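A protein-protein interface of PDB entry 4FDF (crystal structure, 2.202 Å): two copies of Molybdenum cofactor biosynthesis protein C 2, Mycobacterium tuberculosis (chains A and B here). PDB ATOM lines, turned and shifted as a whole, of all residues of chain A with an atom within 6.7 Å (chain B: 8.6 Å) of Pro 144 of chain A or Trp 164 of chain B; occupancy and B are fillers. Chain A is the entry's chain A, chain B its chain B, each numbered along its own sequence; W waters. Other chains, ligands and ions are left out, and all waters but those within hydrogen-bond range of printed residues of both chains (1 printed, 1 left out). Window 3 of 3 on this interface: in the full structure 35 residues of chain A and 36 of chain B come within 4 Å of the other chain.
No position is printed for both chains.
Water W1 lies within hydrogen-bond range of the side-chain carboxylate (OE1) of Glu 121 of chain B (3.0 Å), the side-chain amino group (NZ) of Lys 156 of chain B (3.0 Å) and the side-chain hydroxyl (OH) of Tyr 136 of chain A (3.0 Å).
Printed residues of chain B within 4 Å of Pro 144 of chain A: Lys 156 (3.96 Å) and Trp 164 (3.9 Å). Printed residues of chain B within 4 Å of Leu 147 of chain A: Ile 151 (3.8 Å) and Arg 152 (3.6 Å). Of the printed residues of chain A, Val 153 of chain B touches Tyr 136 (3.3 Å). Trp 164 of chain B touches one residue of chain A. The nearest residue of chain A that does not touch Trp 164 of chain B is Gly 145 of chain A (4.2 Å).
The backbone carbonyl oxygen (O) of Val 153 of chain B lies within hydrogen-bond range of the guanidinium group (NE) of Arg 166 of chain B, 2.7 Å away. A ring nitrogen (ND1) of His 155 of chain B lies close to the backbone carbonyl oxygen of Trp 164 of chain B, at 3.4 Å. The backbone NH of Lys 156 of chain B lies within hydrogen-bond range of the backbone carbonyl oxygen of Trp 164 of chain B, 2.9 Å away. The backbone carbonyl oxygen of Leu 154 of chain B lies within hydrogen-bond range of the backbone NH of Arg 166 of chain B (3.0 Å). The backbone carbonyl oxygen (O) of Pro 144 of chain A is in hydrogen-bond range of the side-chain hydroxyl (OH) of Tyr 136 of chain A (2.8 Å).
O of Gly 145 of chain A sits at hydrogen-bond distance from NH2 of Arg 166 of chain B (3.2 Å).
Among the printed residues, pairs that only touch across the chains: Tyr 136 of chain A with Val 153 of chain B (3.3 Å), Tyr 136 of chain A with Leu 125 of chain B (3.4 Å), Lys 140 of chain A with Glu 121 of chain B (3.4 Å), Leu 147 of chain A with Arg 152 of chain B (3.6 Å), Leu 147 of chain A with Ile 151 of chain B (3.8 Å), Pro 144 of chain A with Trp 164 of chain B (3.9 Å) and Pro 144 of chain A with Lys 156 of chain B (3.96 Å).
Hydrophobic or aromatic side chains of chain A that line the printed part of chain B: Tyr 136, Pro 144 and Leu 147. Of the 17 printed residues of chain B, 8 touch a printed residue of chain A. Along chain B the printed residues that touch a printed residue of chain A span positions 121 to 166.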
ATOM      1  N   TYR A 136      33.136  12.333 -24.468  1.00  0.00           N
ATOM      2  CA  TYR A 136      31.839  12.002 -25.060  1.00  0.00           C
ATOM      3  C   TYR A 136      30.698  12.591 -24.244  1.00  0.00           C
ATOM      4  O   TYR A 136      29.724  13.104 -24.797  1.00  0.00           O
ATOM      5  CB  TYR A 136      31.641  10.483 -25.220  1.00  0.00           C
ATOM      6  CG  TYR A 136      30.267  10.170 -25.781  1.00  0.00           C
ATOM      7  CD1 TYR A 136      30.060  10.053 -27.156  1.00  0.00           C
ATOM      8  CD2 TYR A 136      29.169  10.056 -24.946  1.00  0.00           C
ATOM      9  CE1 TYR A 136      28.789   9.815 -27.679  1.00  0.00           C
ATOM     10  CE2 TYR A 136      27.907   9.824 -25.453  1.00  0.00           C
ATOM     11  CZ  TYR A 136      27.723   9.695 -26.819  1.00  0.00           C
ATOM     12  OH  TYR A 136      26.455   9.459 -27.310  1.00  0.00           O
ATOM     13  N   ILE A 139      30.177  16.255 -25.035  1.00  0.00           N
ATOM     14  CA  ILE A 139      29.731  16.572 -26.393  1.00  0.00           C
ATOM     15  C   ILE A 139      28.498  15.822 -26.892  1.00  0.00           C
ATOM     16  O   ILE A 139      28.014  16.106 -27.993  1.00  0.00           O
ATOM     17  CB  ILE A 139      30.842  16.301 -27.413  1.00  0.00           C
ATOM     18  CG1 ILE A 139      31.095  14.780 -27.500  1.00  0.00           C
ATOM     19  CG2 ILE A 139      32.082  17.108 -27.051  1.00  0.00           C
ATOM     20  CD1 ILE A 139      31.884  14.330 -28.692  1.00  0.00           C
ATOM     21  N   LYS A 140      27.996  14.873 -26.104  1.00  0.00           N
ATOM     22  CA  LYS A 140      26.896  14.001 -26.555  1.00  0.00           C
ATOM     23  C   LYS A 140      25.623  14.733 -27.026  1.00  0.00           C
ATOM     24  O   LYS A 140      24.892  14.223 -27.884  1.00  0.00           O
ATOM     25  CB  LYS A 140      26.558  12.947 -25.489  1.00  0.00           C
ATOM     26  CG  LYS A 140      25.938  13.506 -24.209  1.00  0.00           C
ATOM     27  CD  LYS A 140      25.578  12.398 -23.247  1.00  0.00           C
ATOM     28  CE  LYS A 140      24.825  12.951 -22.058  1.00  0.00           C
ATOM     29  NZ  LYS A 140      25.734  13.665 -21.132  1.00  0.00           N
ATOM     30  N   ALA A 141      25.356  15.916 -26.470  1.00  0.00           N
ATOM     31  CA  ALA A 141      24.193  16.700 -26.891  1.00  0.00           C
ATOM     32  C   ALA A 141      24.401  17.349 -28.259  1.00  0.00           C
ATOM     33  O   ALA A 141      23.432  17.701 -28.941  1.00  0.00           O
ATOM     34  CB  ALA A 141      23.824  17.758 -25.840  1.00  0.00           C
ATOM     35  N   VAL A 142      25.664  17.505 -28.650  1.00  0.00           N
ATOM     36  CA  VAL A 142      26.014  18.086 -29.944  1.00  0.00           C
ATOM     37  C   VAL A 142      26.238  16.996 -30.995  1.00  0.00           C
ATOM     38  O   VAL A 142      25.834  17.159 -32.147  1.00  0.00           O
ATOM     39  CB  VAL A 142      27.254  19.035 -29.853  1.00  0.00           C
ATOM     40  CG1 VAL A 142      27.637  19.577 -31.231  1.00  0.00           C
ATOM     41  CG2 VAL A 142      26.978  20.210 -28.914  1.00  0.00           C
ATOM     42  N   ASP A 143      26.870  15.889 -30.595  1.00  0.00           N
ATOM     43  CA  ASP A 143      27.186  14.796 -31.515  1.00  0.00           C
ATOM     44  C   ASP A 143      26.990  13.429 -30.852  1.00  0.00           C
ATOM     45  O   ASP A 143      27.948  12.798 -30.426  1.00  0.00           O
ATOM     46  CB  ASP A 143      28.614  14.941 -32.054  1.00  0.00           C
ATOM     47  CG  ASP A 143      28.903  14.009 -33.227  1.00  0.00           C
ATOM     48  OD1 ASP A 143      27.994  13.763 -34.040  1.00  0.00           O
ATOM     49  OD2 ASP A 143      30.047  13.518 -33.344  1.00  0.00           O
ATOM     50  N   PRO A 144      25.736  12.962 -30.780  1.00  0.00           N
ATOM     51  CA  PRO A 144      25.436  11.713 -30.078  1.00  0.00           C
ATOM     52  C   PRO A 144      26.011  10.470 -30.766  1.00  0.00           C
ATOM     53  O   PRO A 144      26.245   9.457 -30.105  1.00  0.00           O
ATOM     54  CB  PRO A 144      23.905  11.694 -30.041  1.00  0.00           C
ATOM     55  CG  PRO A 144      23.494  12.536 -31.192  1.00  0.00           C
ATOM     56  CD  PRO A 144      24.516  13.617 -31.285  1.00  0.00           C
ATOM     57  N   GLY A 145      26.280  10.559 -32.065  1.00  0.00           N
ATOM     58  CA  GLY A 145      26.894   9.450 -32.790  1.00  0.00           C
ATOM     59  C   GLY A 145      28.405   9.330 -32.661  1.00  0.00           C
ATOM     60  O   GLY A 145      29.001   8.401 -33.211  1.00  0.00           O
ATOM     61  N   ALA A 146      29.031  10.265 -31.943  1.00  0.00           N
ATOM     62  CA  ALA A 146      30.481  10.221 -31.717  1.00  0.00           C
ATOM     63  C   ALA A 146      30.960   8.831 -31.252  1.00  0.00           C
ATOM     64  O   ALA A 146      30.280   8.177 -30.450  1.00  0.00           O
ATOM     65  CB  ALA A 146      30.887  11.301 -30.722  1.00  0.00           C
ATOM     66  N   LEU A 147      32.115   8.394 -31.763  1.00  0.00           N
ATOM     67  CA  LEU A 147      32.667   7.031 -31.548  1.00  0.00           C
ATOM     68  C   LEU A 147      33.939   7.078 -30.726  1.00  0.00           C
ATOM     69  O   LEU A 147      34.700   8.048 -30.837  1.00  0.00           O
ATOM     70  CB  LEU A 147      33.058   6.393 -32.894  1.00  0.00           C
ATOM     71  CG  LEU A 147      31.998   5.769 -33.803  1.00  0.00           C
ATOM     72  CD1 LEU A 147      32.426   5.813 -35.266  1.00  0.00           C
ATOM     73  CD2 LEU A 147      31.760   4.343 -33.387  1.00  0.00           C
ATOM     74  N   THR B  38      15.452   3.742 -21.662  1.00  0.00           N
ATOM     75  CA  THR B  38      16.376   2.667 -21.979  1.00  0.00           C
ATOM     76  C   THR B  38      17.444   3.109 -22.981  1.00  0.00           C
ATOM     77  O   THR B  38      17.160   3.832 -23.952  1.00  0.00           O
ATOM     78  CB  THR B  38      15.650   1.361 -22.416  1.00  0.00           C
ATOM     79  OG1 THR B  38      16.595   0.460 -23.020  1.00  0.00           O
ATOM     80  CG2 THR B  38      14.540   1.652 -23.393  1.00  0.00           C
ATOM     81  N   ALA B  39      18.680   2.689 -22.722  1.00  0.00           N
ATOM     82  CA  ALA B  39      19.772   2.952 -23.649  1.00  0.00           C
ATOM     83  C   ALA B  39      20.557   1.688 -23.924  1.00  0.00           C
ATOM     84  O   ALA B  39      20.729   0.847 -23.043  1.00  0.00           O
ATOM     85  CB  ALA B  39      20.684   4.043 -23.119  1.00  0.00           C
ATOM     86  N   VAL B  40      21.029   1.570 -25.160  1.00  0.00           N
ATOM     87  CA  VAL B  40      21.841   0.449 -25.594  1.00  0.00           C
ATOM     88  C   VAL B  40      23.130   0.966 -26.239  1.00  0.00           C
ATOM     89  O   VAL B  40      23.109   1.836 -27.131  1.00  0.00           O
ATOM     90  CB  VAL B  40      21.072  -0.475 -26.600  1.00  0.00           C
ATOM     91  CG1 VAL B  40      21.897  -1.729 -26.943  1.00  0.00           C
ATOM     92  CG2 VAL B  40      19.710  -0.879 -26.042  1.00  0.00           C
ATOM     93  N   ALA B  41      24.247   0.415 -25.788  1.00  0.00           N
ATOM     94  CA  ALA B  41      25.549   0.749 -26.337  1.00  0.00           C
ATOM     95  C   ALA B  41      26.260  -0.542 -26.731  1.00  0.00           C
ATOM     96  O   ALA B  41      25.950  -1.601 -26.194  1.00  0.00           O
ATOM     97  CB  ALA B  41      26.368   1.516 -25.310  1.00  0.00           C
ATOM     98  N   GLU B 121      22.529   6.760 -21.523  1.00  0.00           N
ATOM     99  CA  GLU B 121      23.524   6.312 -22.490  1.00  0.00           C
ATOM    100  C   GLU B 121      24.950   6.292 -21.929  1.00  0.00           C
ATOM    101  O   GLU B 121      25.768   5.490 -22.371  1.00  0.00           O
ATOM    102  CB  GLU B 121      23.433   7.092 -23.809  1.00  0.00           C
ATOM    103  CG  GLU B 121      23.805   8.576 -23.746  1.00  0.00           C
ATOM    104  CD  GLU B 121      22.634   9.501 -23.437  1.00  0.00           C
ATOM    105  OE1 GLU B 121      22.681  10.664 -23.882  1.00  0.00           O
ATOM    106  OE2 GLU B 121      21.682   9.089 -22.740  1.00  0.00           O
ATOM    107  N   LEU B 125      27.464   3.060 -22.060  1.00  0.00           N
ATOM    108  CA  LEU B 125      28.821   3.179 -22.620  1.00  0.00           C
ATOM    109  C   LEU B 125      29.921   2.788 -21.618  1.00  0.00           C
ATOM    110  O   LEU B 125      30.914   2.152 -21.990  1.00  0.00           O
ATOM    111  CB  LEU B 125      29.066   4.603 -23.118  1.00  0.00           C
ATOM    112  CG  LEU B 125      28.297   5.047 -24.358  1.00  0.00           C
ATOM    113  CD1 LEU B 125      28.309   6.574 -24.440  1.00  0.00           C
ATOM    114  CD2 LEU B 125      28.853   4.424 -25.637  1.00  0.00           C
ATOM    115  N   ILE B 151      33.276   1.634 -29.715  1.00  0.00           N
ATOM    116  CA  ILE B 151      32.376   1.883 -28.597  1.00  0.00           C
ATOM    117  C   ILE B 151      31.419   3.017 -28.963  1.00  0.00           C
ATOM    118  O   ILE B 151      31.848   4.129 -29.237  1.00  0.00           O
ATOM    119  CB  ILE B 151      33.153   2.204 -27.301  1.00  0.00           C
ATOM    120  CG1 ILE B 151      33.908   0.951 -26.845  1.00  0.00           C
ATOM    121  CG2 ILE B 151      32.192   2.739 -26.205  1.00  0.00           C
ATOM    122  CD1 ILE B 151      35.019   1.209 -25.845  1.00  0.00           C
ATOM    123  N   ARG B 152      30.123   2.733 -28.958  1.00  0.00           N
ATOM    124  CA  ARG B 152      29.152   3.681 -29.485  1.00  0.00           C
ATOM    125  C   ARG B 152      27.748   3.429 -28.947  1.00  0.00           C
ATOM    126  O   ARG B 152      27.419   2.325 -28.484  1.00  0.00           O
ATOM    127  CB  ARG B 152      29.147   3.625 -31.019  1.00  0.00           C
ATOM    128  CG  ARG B 152      28.473   2.376 -31.575  1.00  0.00           C
ATOM    129  CD  ARG B 152      29.267   1.724 -32.698  1.00  0.00           C
ATOM    130  NE  ARG B 152      28.537   0.581 -33.241  1.00  0.00           N
ATOM    131  CZ  ARG B 152      28.706  -0.691 -32.873  1.00  0.00           C
ATOM    132  NH1 ARG B 152      29.609  -1.045 -31.959  1.00  0.00           N
ATOM    133  NH2 ARG B 152      27.963  -1.625 -33.440  1.00  0.00           N
ATOM    134  N   VAL B 153      26.924   4.469 -29.005  1.00  0.00           N
ATOM    135  CA  VAL B 153      25.509   4.347 -28.652  1.00  0.00           C
ATOM    136  C   VAL B 153      24.730   3.751 -29.820  1.00  0.00           C
ATOM    137  O   VAL B 153      24.846   4.202 -30.961  1.00  0.00           O
ATOM    138  CB  VAL B 153      24.903   5.703 -28.243  1.00  0.00           C
ATOM    139  CG1 VAL B 153      23.382   5.584 -28.013  1.00  0.00           C
ATOM    140  CG2 VAL B 153      25.611   6.247 -26.984  1.00  0.00           C
ATOM    141  N   LEU B 154      23.942   2.729 -29.523  1.00  0.00           N
ATOM    142  CA  LEU B 154      23.124   2.055 -30.528  1.00  0.00           C
ATOM    143  C   LEU B 154      21.688   2.546 -30.563  1.00  0.00           C
ATOM    144  O   LEU B 154      21.055   2.554 -31.626  1.00  0.00           O
ATOM    145  CB  LEU B 154      23.122   0.547 -30.265  1.00  0.00           C
ATOM    146  CG  LEU B 154      24.013  -0.367 -31.104  1.00  0.00           C
ATOM    147  CD1 LEU B 154      25.394   0.223 -31.390  1.00  0.00           C
ATOM    148  CD2 LEU B 154      24.102  -1.731 -30.448  1.00  0.00           C
ATOM    149  N   HIS B 155      21.179   2.960 -29.408  1.00  0.00           N
ATOM    150  CA  HIS B 155      19.753   3.162 -29.227  1.00  0.00           C
ATOM    151  C   HIS B 155      19.472   3.862 -27.922  1.00  0.00           C
ATOM    152  O   HIS B 155      20.096   3.551 -26.901  1.00  0.00           O
ATOM    153  CB  HIS B 155      19.054   1.800 -29.263  1.00  0.00           C
ATOM    154  CG  HIS B 155      17.556   1.872 -29.184  1.00  0.00           C
ATOM    155  ND1 HIS B 155      16.777   1.965 -30.280  1.00  0.00           N
ATOM    156  CD2 HIS B 155      16.693   1.852 -28.084  1.00  0.00           C
ATOM    157  CE1 HIS B 155      15.480   2.007 -29.906  1.00  0.00           C
ATOM    158  NE2 HIS B 155      15.431   1.941 -28.561  1.00  0.00           N
ATOM    159  N   LYS B 156      18.538   4.819 -27.959  1.00  0.00           N
ATOM    160  CA  LYS B 156      18.026   5.513 -26.777  1.00  0.00           C
ATOM    161  C   LYS B 156      16.518   5.675 -26.912  1.00  0.00           C
ATOM    162  O   LYS B 156      16.019   6.080 -27.969  1.00  0.00           O
ATOM    163  CB  LYS B 156      18.637   6.905 -26.616  1.00  0.00           C
ATOM    164  CG  LYS B 156      20.151   6.964 -26.472  1.00  0.00           C
ATOM    165  CD  LYS B 156      20.627   8.419 -26.418  1.00  0.00           C
ATOM    166  CE  LYS B 156      20.592   9.069 -27.800  1.00  0.00           C
ATOM    167  NZ  LYS B 156      20.885  10.538 -27.751  1.00  0.00           N
ATOM    168  N   GLU B 157      15.799   5.383 -25.832  1.00  0.00           N
ATOM    169  CA  GLU B 157      14.340   5.360 -25.852  1.00  0.00           C
ATOM    170  C   GLU B 157      13.764   5.841 -24.519  1.00  0.00           C
ATOM    171  O   GLU B 157      12.640   6.349 -24.458  1.00  0.00           O
ATOM    172  CB  GLU B 157      13.873   3.938 -26.156  1.00  0.00           C
ATOM    173  CG  GLU B 157      12.442   3.797 -26.628  1.00  0.00           C
ATOM    174  CD  GLU B 157      12.036   2.339 -26.807  1.00  0.00           C
ATOM    175  OE1 GLU B 157      10.835   2.033 -26.633  1.00  0.00           O
ATOM    176  OE2 GLU B 157      12.912   1.495 -27.114  1.00  0.00           O
ATOM    177  N   THR B 163      12.468   8.720 -30.248  1.00  0.00           N
ATOM    178  CA  THR B 163      13.249   7.487 -30.318  1.00  0.00           C
ATOM    179  C   THR B 163      14.502   7.654 -31.178  1.00  0.00           C
ATOM    180  O   THR B 163      14.434   8.130 -32.318  1.00  0.00           O
ATOM    181  CB  THR B 163      12.387   6.308 -30.813  1.00  0.00           C
ATOM    182  N   TRP B 164      15.638   7.257 -30.612  1.00  0.00           N
ATOM    183  CA  TRP B 164      16.951   7.413 -31.242  1.00  0.00           C
ATOM    184  C   TRP B 164      17.551   6.067 -31.525  1.00  0.00           C
ATOM    185  O   TRP B 164      17.594   5.201 -30.653  1.00  0.00           O
ATOM    186  CB  TRP B 164      17.874   8.211 -30.330  1.00  0.00           C
ATOM    187  CG  TRP B 164      19.072   8.807 -31.028  1.00  0.00           C
ATOM    188  CD1 TRP B 164      19.203  10.096 -31.524  1.00  0.00           C
ATOM    189  CD2 TRP B 164      20.356   8.152 -31.326  1.00  0.00           C
ATOM    190  NE1 TRP B 164      20.434  10.278 -32.094  1.00  0.00           N
ATOM    191  CE2 TRP B 164      21.176   9.155 -32.002  1.00  0.00           C
ATOM    192  CE3 TRP B 164      20.884   6.876 -31.112  1.00  0.00           C
ATOM    193  CZ2 TRP B 164      22.465   8.879 -32.440  1.00  0.00           C
ATOM    194  CZ3 TRP B 164      22.191   6.611 -31.550  1.00  0.00           C
ATOM    195  CH2 TRP B 164      22.960   7.590 -32.200  1.00  0.00           C
ATOM    196  N   THR B 165      18.023   5.878 -32.752  1.00  0.00           N
ATOM    197  CA  THR B 165      18.603   4.607 -33.163  1.00  0.00           C
ATOM    198  C   THR B 165      19.657   4.852 -34.234  1.00  0.00           C
ATOM    199  O   THR B 165      19.422   5.593 -35.189  1.00  0.00           O
ATOM    200  CB  THR B 165      17.508   3.593 -33.636  1.00  0.00           C
ATOM    201  OG1 THR B 165      18.116   2.398 -34.137  1.00  0.00           O
ATOM    202  CG2 THR B 165      16.623   4.191 -34.718  1.00  0.00           C
ATOM    203  N   ARG B 166      20.825   4.245 -34.057  1.00  0.00           N
ATOM    204  CA  ARG B 166      21.944   4.457 -34.966  1.00  0.00           C
ATOM    205  C   ARG B 166      21.657   3.873 -36.356  1.00  0.00           C
ATOM    206  O   ARG B 166      21.100   2.782 -36.496  1.00  0.00           O
ATOM    207  CB  ARG B 166      23.234   3.872 -34.376  1.00  0.00           C
ATOM    208  CG  ARG B 166      24.451   3.992 -35.280  1.00  0.00           C
ATOM    209  CD  ARG B 166      25.722   3.508 -34.592  1.00  0.00           C
ATOM    210  NE  ARG B 166      26.011   4.345 -33.439  1.00  0.00           N
ATOM    211  CZ  ARG B 166      26.902   5.330 -33.406  1.00  0.00           C
ATOM    212  NH1 ARG B 166      27.660   5.616 -34.462  1.00  0.00           N
ATOM    213  NH2 ARG B 166      27.041   6.023 -32.286  1.00  0.00           N
HETATM  214  O   HOH W   1      23.694  10.580 -26.667  1.00  0.00           O
